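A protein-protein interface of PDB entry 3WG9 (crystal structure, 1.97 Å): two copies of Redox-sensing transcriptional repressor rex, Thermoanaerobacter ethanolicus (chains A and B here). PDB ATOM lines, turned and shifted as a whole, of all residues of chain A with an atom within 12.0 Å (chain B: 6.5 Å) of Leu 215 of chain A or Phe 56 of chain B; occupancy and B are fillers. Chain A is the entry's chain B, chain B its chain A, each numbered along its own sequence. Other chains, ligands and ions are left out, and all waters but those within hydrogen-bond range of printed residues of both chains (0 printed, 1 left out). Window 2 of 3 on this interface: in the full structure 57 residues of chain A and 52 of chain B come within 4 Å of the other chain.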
ATOM      1  N   PHE A 200      17.584   4.998  28.986  1.00  0.00           N
ATOM      2  CA  PHE A 200      17.600   4.285  27.699  1.00  0.00           C
ATOM      3  C   PHE A 200      18.501   3.074  27.704  1.00  0.00           C
ATOM      4  O   PHE A 200      18.428   2.238  26.799  1.00  0.00           O
ATOM      5  CB  PHE A 200      17.916   5.167  26.500  1.00  0.00           C
ATOM      6  CG  PHE A 200      16.888   6.212  26.247  1.00  0.00           C
ATOM      7  CD1 PHE A 200      15.661   6.201  26.924  1.00  0.00           C
ATOM      8  CD2 PHE A 200      17.161   7.245  25.373  1.00  0.00           C
ATOM      9  CE1 PHE A 200      14.702   7.184  26.686  1.00  0.00           C
ATOM     10  CE2 PHE A 200      16.196   8.234  25.107  1.00  0.00           C
ATOM     11  CZ  PHE A 200      14.963   8.206  25.777  1.00  0.00           C
ATOM     12  N   THR A 201      19.389   2.964  28.694  1.00  0.00           N
ATOM     13  CA  THR A 201      20.102   1.702  28.821  1.00  0.00           C
ATOM     14  C   THR A 201      19.287   0.599  29.400  1.00  0.00           C
ATOM     15  O   THR A 201      19.636  -0.570  29.225  1.00  0.00           O
ATOM     16  CB  THR A 201      21.457   1.799  29.669  1.00  0.00           C
ATOM     17  OG1 THR A 201      21.126   1.957  31.053  1.00  0.00           O
ATOM     18  CG2 THR A 201      22.338   3.010  29.190  1.00  0.00           C
ATOM     19  N   SER A 203      15.975   0.243  28.545  1.00  0.00           N
ATOM     20  CA  SER A 203      15.276  -0.264  27.355  1.00  0.00           C
ATOM     21  C   SER A 203      16.238  -1.121  26.504  1.00  0.00           C
ATOM     22  O   SER A 203      15.837  -2.151  25.911  1.00  0.00           O
ATOM     23  CB  SER A 203      14.643   0.867  26.549  1.00  0.00           C
ATOM     24  OG  SER A 203      15.528   1.968  26.438  1.00  0.00           O
ATOM     25  N   TYR A 204      17.494  -0.687  26.425  1.00  0.00           N
ATOM     26  CA  TYR A 204      18.452  -1.429  25.624  1.00  0.00           C
ATOM     27  C   TYR A 204      18.621  -2.844  26.140  1.00  0.00           C
ATOM     28  O   TYR A 204      18.527  -3.835  25.367  1.00  0.00           O
ATOM     29  CB  TYR A 204      19.781  -0.699  25.496  1.00  0.00           C
ATOM     30  CG  TYR A 204      20.790  -1.578  24.775  1.00  0.00           C
ATOM     31  CD1 TYR A 204      21.182  -1.314  23.468  1.00  0.00           C
ATOM     32  CD2 TYR A 204      21.368  -2.647  25.425  1.00  0.00           C
ATOM     33  CE1 TYR A 204      22.123  -2.155  22.813  1.00  0.00           C
ATOM     34  CE2 TYR A 204      22.282  -3.486  24.796  1.00  0.00           C
ATOM     35  CZ  TYR A 204      22.667  -3.221  23.503  1.00  0.00           C
ATOM     36  OH  TYR A 204      23.615  -4.064  22.922  1.00  0.00           O
ATOM     37  N   ARG A 205      18.733  -2.965  27.459  1.00  0.00           N
ATOM     38  CA  ARG A 205      19.018  -4.260  28.048  1.00  0.00           C
ATOM     39  C   ARG A 205      17.835  -5.192  28.102  1.00  0.00           C
ATOM     40  O   ARG A 205      18.020  -6.417  28.002  1.00  0.00           O
ATOM     41  CB  ARG A 205      19.616  -4.110  29.450  1.00  0.00           C
ATOM     42  CG  ARG A 205      21.049  -3.624  29.395  1.00  0.00           C
ATOM     43  CD  ARG A 205      21.590  -3.421  30.816  1.00  0.00           C
ATOM     44  NE  ARG A 205      21.393  -2.022  31.183  1.00  0.00           N
ATOM     45  CZ  ARG A 205      21.778  -1.533  32.358  1.00  0.00           C
ATOM     46  NH1 ARG A 205      22.370  -2.360  33.231  1.00  0.00           N
ATOM     47  NH2 ARG A 205      21.610  -0.250  32.643  1.00  0.00           N
ATOM     48  N   LEU A 206      16.622  -4.637  28.222  1.00  0.00           N
ATOM     49  CA  LEU A 206      15.406  -5.432  28.096  1.00  0.00           C
ATOM     50  C   LEU A 206      15.253  -6.052  26.703  1.00  0.00           C
ATOM     51  O   LEU A 206      14.551  -7.042  26.536  1.00  0.00           O
ATOM     52  CB  LEU A 206      14.152  -4.568  28.385  1.00  0.00           C
ATOM     53  CG  LEU A 206      13.919  -4.237  29.870  1.00  0.00           C
ATOM     54  CD1 LEU A 206      12.899  -3.134  30.043  1.00  0.00           C
ATOM     55  CD2 LEU A 206      13.527  -5.447  30.679  1.00  0.00           C
ATOM     56  N   ASN A 207      15.900  -5.480  25.696  1.00  0.00           N
ATOM     57  CA  ASN A 207      15.723  -5.952  24.311  1.00  0.00           C
ATOM     58  C   ASN A 207      16.922  -6.547  23.672  1.00  0.00           C
ATOM     59  O   ASN A 207      16.845  -6.995  22.513  1.00  0.00           O
ATOM     60  CB  ASN A 207      15.235  -4.812  23.409  1.00  0.00           C
ATOM     61  CG  ASN A 207      13.825  -4.477  23.695  1.00  0.00           C
ATOM     62  OD1 ASN A 207      12.926  -5.281  23.458  1.00  0.00           O
ATOM     63  ND2 ASN A 207      13.618  -3.326  24.317  1.00  0.00           N
ATOM     64  N   GLU A 208      18.029  -6.561  24.389  1.00  0.00           N
ATOM     65  CA  GLU A 208      19.256  -6.956  23.741  1.00  0.00           C
ATOM     66  C   GLU A 208      19.182  -8.381  23.142  1.00  0.00           C
ATOM     67  O   GLU A 208      19.636  -8.598  22.000  1.00  0.00           O
ATOM     68  CB  GLU A 208      20.444  -6.887  24.677  1.00  0.00           C
ATOM     69  CG  GLU A 208      21.758  -7.080  23.906  1.00  0.00           C
ATOM     70  CD  GLU A 208      23.011  -6.975  24.767  1.00  0.00           C
ATOM     71  OE1 GLU A 208      23.058  -7.626  25.812  1.00  0.00           O
ATOM     72  OE2 GLU A 208      23.918  -6.195  24.418  1.00  0.00           O
ATOM     73  N   GLU A 209      18.656  -9.337  23.906  1.00  0.00           N
ATOM     74  CA  GLU A 209      18.769 -10.723  23.453  1.00  0.00           C
ATOM     75  C   GLU A 209      17.902 -10.872  22.223  1.00  0.00           C
ATOM     76  O   GLU A 209      18.324 -11.470  21.238  1.00  0.00           O
ATOM     77  CB  GLU A 209      18.372 -11.747  24.526  1.00  0.00           C
ATOM     78  CG  GLU A 209      17.040 -11.419  25.176  1.00  0.00           C
ATOM     79  CD  GLU A 209      16.149 -12.634  25.469  1.00  0.00           C
ATOM     80  OE1 GLU A 209      16.683 -13.726  25.802  1.00  0.00           O
ATOM     81  OE2 GLU A 209      14.898 -12.453  25.394  1.00  0.00           O
ATOM     82  N   GLU A 210      16.698 -10.312  22.268  1.00  0.00           N
ATOM     83  CA  GLU A 210      15.911 -10.195  21.072  1.00  0.00           C
ATOM     84  C   GLU A 210      16.709  -9.602  19.912  1.00  0.00           C
ATOM     85  O   GLU A 210      16.754 -10.183  18.822  1.00  0.00           O
ATOM     86  CB  GLU A 210      14.638  -9.410  21.346  1.00  0.00           C
ATOM     87  CG  GLU A 210      13.511  -9.717  20.369  1.00  0.00           C
ATOM     88  CD  GLU A 210      12.549  -8.548  20.168  1.00  0.00           C
ATOM     89  OE1 GLU A 210      12.991  -7.367  20.204  1.00  0.00           O
ATOM     90  OE2 GLU A 210      11.345  -8.804  19.926  1.00  0.00           O
ATOM     91  N   LEU A 211      17.336  -8.456  20.124  1.00  0.00           N
ATOM     92  CA  LEU A 211      18.022  -7.742  19.054  1.00  0.00           C
ATOM     93  C   LEU A 211      19.027  -8.640  18.338  1.00  0.00           C
ATOM     94  O   LEU A 211      19.167  -8.564  17.116  1.00  0.00           O
ATOM     95  CB  LEU A 211      18.754  -6.525  19.613  1.00  0.00           C
ATOM     96  CG  LEU A 211      19.659  -5.627  18.772  1.00  0.00           C
ATOM     97  CD1 LEU A 211      18.876  -4.954  17.631  1.00  0.00           C
ATOM     98  CD2 LEU A 211      20.372  -4.547  19.672  1.00  0.00           C
ATOM     99  N   PHE A 212      19.773  -9.426  19.105  1.00  0.00           N
ATOM    100  CA  PHE A 212      20.769 -10.326  18.541  1.00  0.00           C
ATOM    101  C   PHE A 212      20.200 -11.683  18.134  1.00  0.00           C
ATOM    102  O   PHE A 212      20.944 -12.502  17.627  1.00  0.00           O
ATOM    103  CB  PHE A 212      21.941 -10.520  19.508  1.00  0.00           C
ATOM    104  CG  PHE A 212      22.837  -9.353  19.565  1.00  0.00           C
ATOM    105  CD1 PHE A 212      23.876  -9.221  18.663  1.00  0.00           C
ATOM    106  CD2 PHE A 212      22.583  -8.308  20.456  1.00  0.00           C
ATOM    107  CE1 PHE A 212      24.682  -8.099  18.683  1.00  0.00           C
ATOM    108  CE2 PHE A 212      23.389  -7.194  20.491  1.00  0.00           C
ATOM    109  CZ  PHE A 212      24.451  -7.075  19.624  1.00  0.00           C
ATOM    110  N   LYS A 213      18.939 -11.953  18.457  1.00  0.00           N
ATOM    111  CA  LYS A 213      18.215 -13.120  17.969  1.00  0.00           C
ATOM    112  C   LYS A 213      17.573 -12.697  16.640  1.00  0.00           C
ATOM    113  O   LYS A 213      17.656 -13.411  15.647  1.00  0.00           O
ATOM    114  CB  LYS A 213      17.085 -13.491  18.932  1.00  0.00           C
ATOM    115  CG  LYS A 213      17.190 -14.779  19.750  1.00  0.00           C
ATOM    116  CD  LYS A 213      15.816 -15.056  20.397  1.00  0.00           C
ATOM    117  CE  LYS A 213      15.359 -13.849  21.256  1.00  0.00           C
ATOM    118  NZ  LYS A 213      13.941 -13.340  21.084  1.00  0.00           N
ATOM    119  N   LYS A 214      16.922 -11.536  16.635  1.00  0.00           N
ATOM    120  CA  LYS A 214      16.481 -10.864  15.405  1.00  0.00           C
ATOM    121  C   LYS A 214      17.640 -10.824  14.405  1.00  0.00           C
ATOM    122  O   LYS A 214      17.855 -11.786  13.649  1.00  0.00           O
ATOM    123  CB  LYS A 214      16.009  -9.428  15.713  1.00  0.00           C
ATOM    124  CG  LYS A 214      14.508  -9.272  15.934  1.00  0.00           C
ATOM    125  CD  LYS A 214      14.035  -7.900  15.461  1.00  0.00           C
ATOM    126  CE  LYS A 214      14.626  -6.759  16.292  1.00  0.00           C
ATOM    127  NZ  LYS A 214      13.665  -6.366  17.352  1.00  0.00           N
ATOM    128  N   LEU A 215      18.394  -9.723  14.430  1.00  0.00           N
ATOM    129  CA  LEU A 215      19.578  -9.535  13.577  1.00  0.00           C
ATOM    130  C   LEU A 215      19.850 -10.693  12.614  1.00  0.00           C
ATOM    131  O   LEU A 215      20.995 -11.116  12.450  1.00  0.00           O
ATOM    132  CB  LEU A 215      20.823  -9.271  14.430  1.00  0.00           C
ATOM    133  CG  LEU A 215      21.286  -7.825  14.499  1.00  0.00           C
ATOM    134  CD1 LEU A 215      22.532  -7.725  15.389  1.00  0.00           C
ATOM    135  CD2 LEU A 215      21.579  -7.302  13.094  1.00  0.00           C
ATOM    136  N   VAL B   7      26.719  -6.901  24.365  1.00  0.00           N
ATOM    137  CA  VAL B   7      27.604  -5.813  23.989  1.00  0.00           C
ATOM    138  C   VAL B   7      28.118  -5.148  25.276  1.00  0.00           C
ATOM    139  O   VAL B   7      27.471  -5.220  26.339  1.00  0.00           O
ATOM    140  CB  VAL B   7      26.891  -4.753  23.125  1.00  0.00           C
ATOM    141  CG1 VAL B   7      27.790  -3.590  22.913  1.00  0.00           C
ATOM    142  CG2 VAL B   7      26.449  -5.319  21.743  1.00  0.00           C
ATOM    143  N   VAL B  11      30.145   0.413  25.678  1.00  0.00           N
ATOM    144  CA  VAL B  11      29.525   0.707  24.364  1.00  0.00           C
ATOM    145  C   VAL B  11      28.056   1.122  24.589  1.00  0.00           C
ATOM    146  O   VAL B  11      27.636   2.161  24.113  1.00  0.00           O
ATOM    147  CB  VAL B  11      29.599  -0.464  23.344  1.00  0.00           C
ATOM    148  CG1 VAL B  11      28.767  -0.122  22.110  1.00  0.00           C
ATOM    149  CG2 VAL B  11      31.078  -0.795  22.897  1.00  0.00           C
ATOM    150  N   ILE B  12      27.319   0.357  25.377  1.00  0.00           N
ATOM    151  CA  ILE B  12      25.879   0.645  25.561  1.00  0.00           C
ATOM    152  C   ILE B  12      25.635   2.085  26.030  1.00  0.00           C
ATOM    153  O   ILE B  12      24.702   2.777  25.548  1.00  0.00           O
ATOM    154  CB  ILE B  12      25.288  -0.389  26.513  1.00  0.00           C
ATOM    155  CG1 ILE B  12      25.304  -1.775  25.862  1.00  0.00           C
ATOM    156  CG2 ILE B  12      23.848  -0.020  27.038  1.00  0.00           C
ATOM    157  CD1 ILE B  12      25.146  -2.903  26.831  1.00  0.00           C
ATOM    158  N   LEU B  15      25.674   4.863  23.333  1.00  0.00           N
ATOM    159  CA  LEU B  15      24.549   4.817  22.364  1.00  0.00           C
ATOM    160  C   LEU B  15      23.460   5.854  22.562  1.00  0.00           C
ATOM    161  O   LEU B  15      22.977   6.440  21.589  1.00  0.00           O
ATOM    162  CB  LEU B  15      23.926   3.414  22.256  1.00  0.00           C
ATOM    163  CG  LEU B  15      24.824   2.246  21.873  1.00  0.00           C
ATOM    164  CD1 LEU B  15      24.035   0.974  21.999  1.00  0.00           C
ATOM    165  CD2 LEU B  15      25.477   2.422  20.462  1.00  0.00           C
ATOM    166  N   GLN B  51      33.353   1.474  15.319  1.00  0.00           N
ATOM    167  CA  GLN B  51      33.419   0.163  15.990  1.00  0.00           C
ATOM    168  C   GLN B  51      32.258  -0.046  16.951  1.00  0.00           C
ATOM    169  O   GLN B  51      31.839  -1.201  17.154  1.00  0.00           O
ATOM    170  CB  GLN B  51      34.730   0.002  16.777  1.00  0.00           C
ATOM    171  CG  GLN B  51      34.775  -1.347  17.529  1.00  0.00           C
ATOM    172  CD  GLN B  51      36.051  -1.516  18.342  1.00  0.00           C
ATOM    173  OE1 GLN B  51      37.065  -0.831  18.099  1.00  0.00           O
ATOM    174  NE2 GLN B  51      36.006  -2.411  19.335  1.00  0.00           N
ATOM    175  N   ASP B  52      31.770   1.043  17.566  1.00  0.00           N
ATOM    176  CA  ASP B  52      30.517   0.967  18.398  1.00  0.00           C
ATOM    177  C   ASP B  52      29.413   0.356  17.493  1.00  0.00           C
ATOM    178  O   ASP B  52      28.846  -0.736  17.746  1.00  0.00           O
ATOM    179  CB  ASP B  52      30.118   2.364  18.997  1.00  0.00           C
ATOM    180  CG  ASP B  52      30.987   2.803  20.197  1.00  0.00           C
ATOM    181  OD1 ASP B  52      31.621   1.923  20.821  1.00  0.00           O
ATOM    182  OD2 ASP B  52      31.095   4.029  20.527  1.00  0.00           O
ATOM    183  N   LEU B  53      29.221   0.987  16.337  1.00  0.00           N
ATOM    184  CA  LEU B  53      28.114   0.626  15.444  1.00  0.00           C
ATOM    185  C   LEU B  53      28.256  -0.765  14.839  1.00  0.00           C
ATOM    186  O   LEU B  53      27.268  -1.523  14.740  1.00  0.00           O
ATOM    187  CB  LEU B  53      27.966   1.698  14.359  1.00  0.00           C
ATOM    188  CG  LEU B  53      27.766   3.057  15.033  1.00  0.00           C
ATOM    189  CD1 LEU B  53      27.774   4.262  14.049  1.00  0.00           C
ATOM    190  CD2 LEU B  53      26.510   3.038  15.946  1.00  0.00           C
ATOM    191  N   ASN B  54      29.510  -1.133  14.521  1.00  0.00           N
ATOM    192  CA  ASN B  54      29.796  -2.458  13.951  1.00  0.00           C
ATOM    193  C   ASN B  54      29.402  -3.592  14.865  1.00  0.00           C
ATOM    194  O   ASN B  54      29.453  -4.772  14.484  1.00  0.00           O
ATOM    195  CB  ASN B  54      31.287  -2.574  13.601  1.00  0.00           C
ATOM    196  CG  ASN B  54      31.623  -1.809  12.349  1.00  0.00           C
ATOM    197  OD1 ASN B  54      32.724  -1.259  12.206  1.00  0.00           O
ATOM    198  ND2 ASN B  54      30.637  -1.717  11.441  1.00  0.00           N
ATOM    199  N   ASN B  55      29.000  -3.236  16.086  1.00  0.00           N
ATOM    200  CA  ASN B  55      28.471  -4.239  16.993  1.00  0.00           C
ATOM    201  C   ASN B  55      27.092  -4.626  16.525  1.00  0.00           C
ATOM    202  O   ASN B  55      26.587  -5.700  16.890  1.00  0.00           O
ATOM    203  CB  ASN B  55      28.387  -3.695  18.440  1.00  0.00           C
ATOM    204  CG  ASN B  55      29.747  -3.578  19.118  1.00  0.00           C
ATOM    205  OD1 ASN B  55      30.286  -4.570  19.624  1.00  0.00           O
ATOM    206  ND2 ASN B  55      30.296  -2.357  19.167  1.00  0.00           N
ATOM    207  N   PHE B  56      26.478  -3.739  15.729  1.00  0.00           N
ATOM    208  CA  PHE B  56      25.073  -3.902  15.326  1.00  0.00           C
ATOM    209  C   PHE B  56      24.885  -4.040  13.800  1.00  0.00           C
ATOM    210  O   PHE B  56      23.763  -4.247  13.357  1.00  0.00           O
ATOM    211  CB  PHE B  56      24.167  -2.778  15.909  1.00  0.00           C
ATOM    212  CG  PHE B  56      24.406  -2.500  17.406  1.00  0.00           C
ATOM    213  CD1 PHE B  56      23.940  -3.373  18.360  1.00  0.00           C
ATOM    214  CD2 PHE B  56      25.195  -1.408  17.812  1.00  0.00           C
ATOM    215  CE1 PHE B  56      24.206  -3.131  19.723  1.00  0.00           C
ATOM    216  CE2 PHE B  56      25.432  -1.147  19.160  1.00  0.00           C
ATOM    217  CZ  PHE B  56      24.950  -2.020  20.099  1.00  0.00           C
ATOM    218  N   GLY B  57      25.977  -3.926  13.029  1.00  0.00           N
ATOM    219  CA  GLY B  57      25.997  -4.179  11.568  1.00  0.00           C
ATOM    220  C   GLY B  57      26.184  -2.921  10.732  1.00  0.00           C
ATOM    221  O   GLY B  57      27.008  -2.051  11.057  1.00  0.00           O
ATOM    222  N   LEU B  75      19.476   3.486  15.625  1.00  0.00           N
ATOM    223  CA  LEU B  75      19.740   3.742  17.062  1.00  0.00           C
ATOM    224  C   LEU B  75      18.460   3.637  17.894  1.00  0.00           C
ATOM    225  O   LEU B  75      18.479   3.060  18.984  1.00  0.00           O
ATOM    226  CB  LEU B  75      20.427   5.096  17.257  1.00  0.00           C
ATOM    227  CG  LEU B  75      21.873   5.137  16.817  1.00  0.00           C
ATOM    228  CD1 LEU B  75      22.408   6.570  16.809  1.00  0.00           C
ATOM    229  CD2 LEU B  75      22.727   4.238  17.716  1.00  0.00           C
ATOM    230  N   ILE B  78      17.777  -0.083  18.186  1.00  0.00           N
ATOM    231  CA  ILE B  78      18.792  -0.719  19.047  1.00  0.00           C
ATOM    232  C   ILE B  78      18.533  -0.435  20.547  1.00  0.00           C
ATOM    233  O   ILE B  78      18.793  -1.277  21.422  1.00  0.00           O
ATOM    234  CB  ILE B  78      20.205  -0.256  18.662  1.00  0.00           C
ATOM    235  CG1 ILE B  78      20.578  -0.785  17.253  1.00  0.00           C
ATOM    236  CG2 ILE B  78      21.222  -0.716  19.681  1.00  0.00           C
ATOM    237  CD1 ILE B  78      21.707   0.046  16.570  1.00  0.00           C
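N of Val 7 of chain B sits at hydrogen-bond distance from OE2 of Glu 208 of chain A, 2.9 Å away.
ND2 of Asn 55 of chain B sits at hydrogen-bond distance from O of Gln 51 of chain B (2.8 Å).
OH of Tyr 204 of chain A is in hydrogen-bond range of OE2 of Glu 208 of chain A (2.6 Å).
O of Asp 52 of chain B is in hydrogen-bond range of ND2 of Asn 55 of chain B, 2.6 Å away.
The side-chain hydroxyl (OG1) of Thr 201 of chain A sits at hydrogen-bond distance from the guanidinium group (NH2) of Arg 205 of chain A, at 2.8 Å.
Thr 201 of chain A touches Ile 12 of chain B (CB to CG2, 3.99 Å).
Tyr 204 of chain A touches Val 7 of chain B.
CE2 of Tyr 204 of chain A touches CD1 of Ile 12 of chain B (3.6 Å).
CE1 of Tyr 204 of chain A touches CD1 of Leu 15 of chain B (3.8 Å).
Tyr 204 of chain A touches Phe 56 of chain B (OH to CE1, 3.4 Å).
CD2 of Leu 211 of chain A touches CD1 of Phe 56 of chain B, at 3.98 Å.
CD2 of Leu 211 of chain A touches CG2 of Ile 78 of chain B (3.9 Å).
Phe 212 of chain A touches Asn 55 of chain B.
Phe 56 of chain B touches Phe 212 of chain A (CD1 to CZ, 3.9 Å).
Leu 215 of chain A touches Phe 56 of chain B.
Leu 215 of chain A touches one residue of chain B.
Of chain A, only Tyr 204 (3.4 Å), Leu 211 (3.98 Å), Phe 212 (3.9 Å) and Leu 215 (3.8 Å) come within 4 Å of Phe 56 of chain B.
Val 7 of chain B touches three residues of chain A.
No residue of chain A comes within 4 Å of Asp 52 of chain B.
No residue of chain A comes within 4 Å of Leu 53 of chain B.
No residue of chain A comes within 4 Å of Asn 54 of chain B.
Of chain A, only Phe 212 comes within 4 Å of Asn 55 of chain B.
No residue of chain A comes within 4 Å of Gly 57 of chain B.
Of the printed residues of chain A, Ile 12 of chain B touches Thr 201 and Tyr 204.
Printed residues of chain B within 4 Å of Tyr 204 of chain A: Val 7 (3.3 Å), Ile 12 (3.6 Å), Leu 15 (3.8 Å), Phe 56 (3.4 Å) and Ile 78 (3.1 Å).
Of the printed residues of chain B, Phe 212 of chain A touches Val 7 (3.4 Å), Asn 55 (3.5 Å) and Phe 56 (3.9 Å).
Of the printed residues of chain A, Leu 15 of chain B touches Tyr 204.
Printed residues of chain B within 4 Å of Thr 201 of chain A: Ile 12.
The nearest residue of chain A that does not touch Phe 56 of chain B is Glu 208 of chain A (5.6 Å).
Of the 15 printed residues of chain A, 6 touch a printed residue of chain B.
Among the printed residues, no Asp or Glu carboxylate lies within 4 Å of a Lys or Arg side-chain nitrogen of the other chain.
No position is printed for both chains.
Of the 13 pairs that touch across the chains among the printed residues, none has its exchanged pair printed and touching as well.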
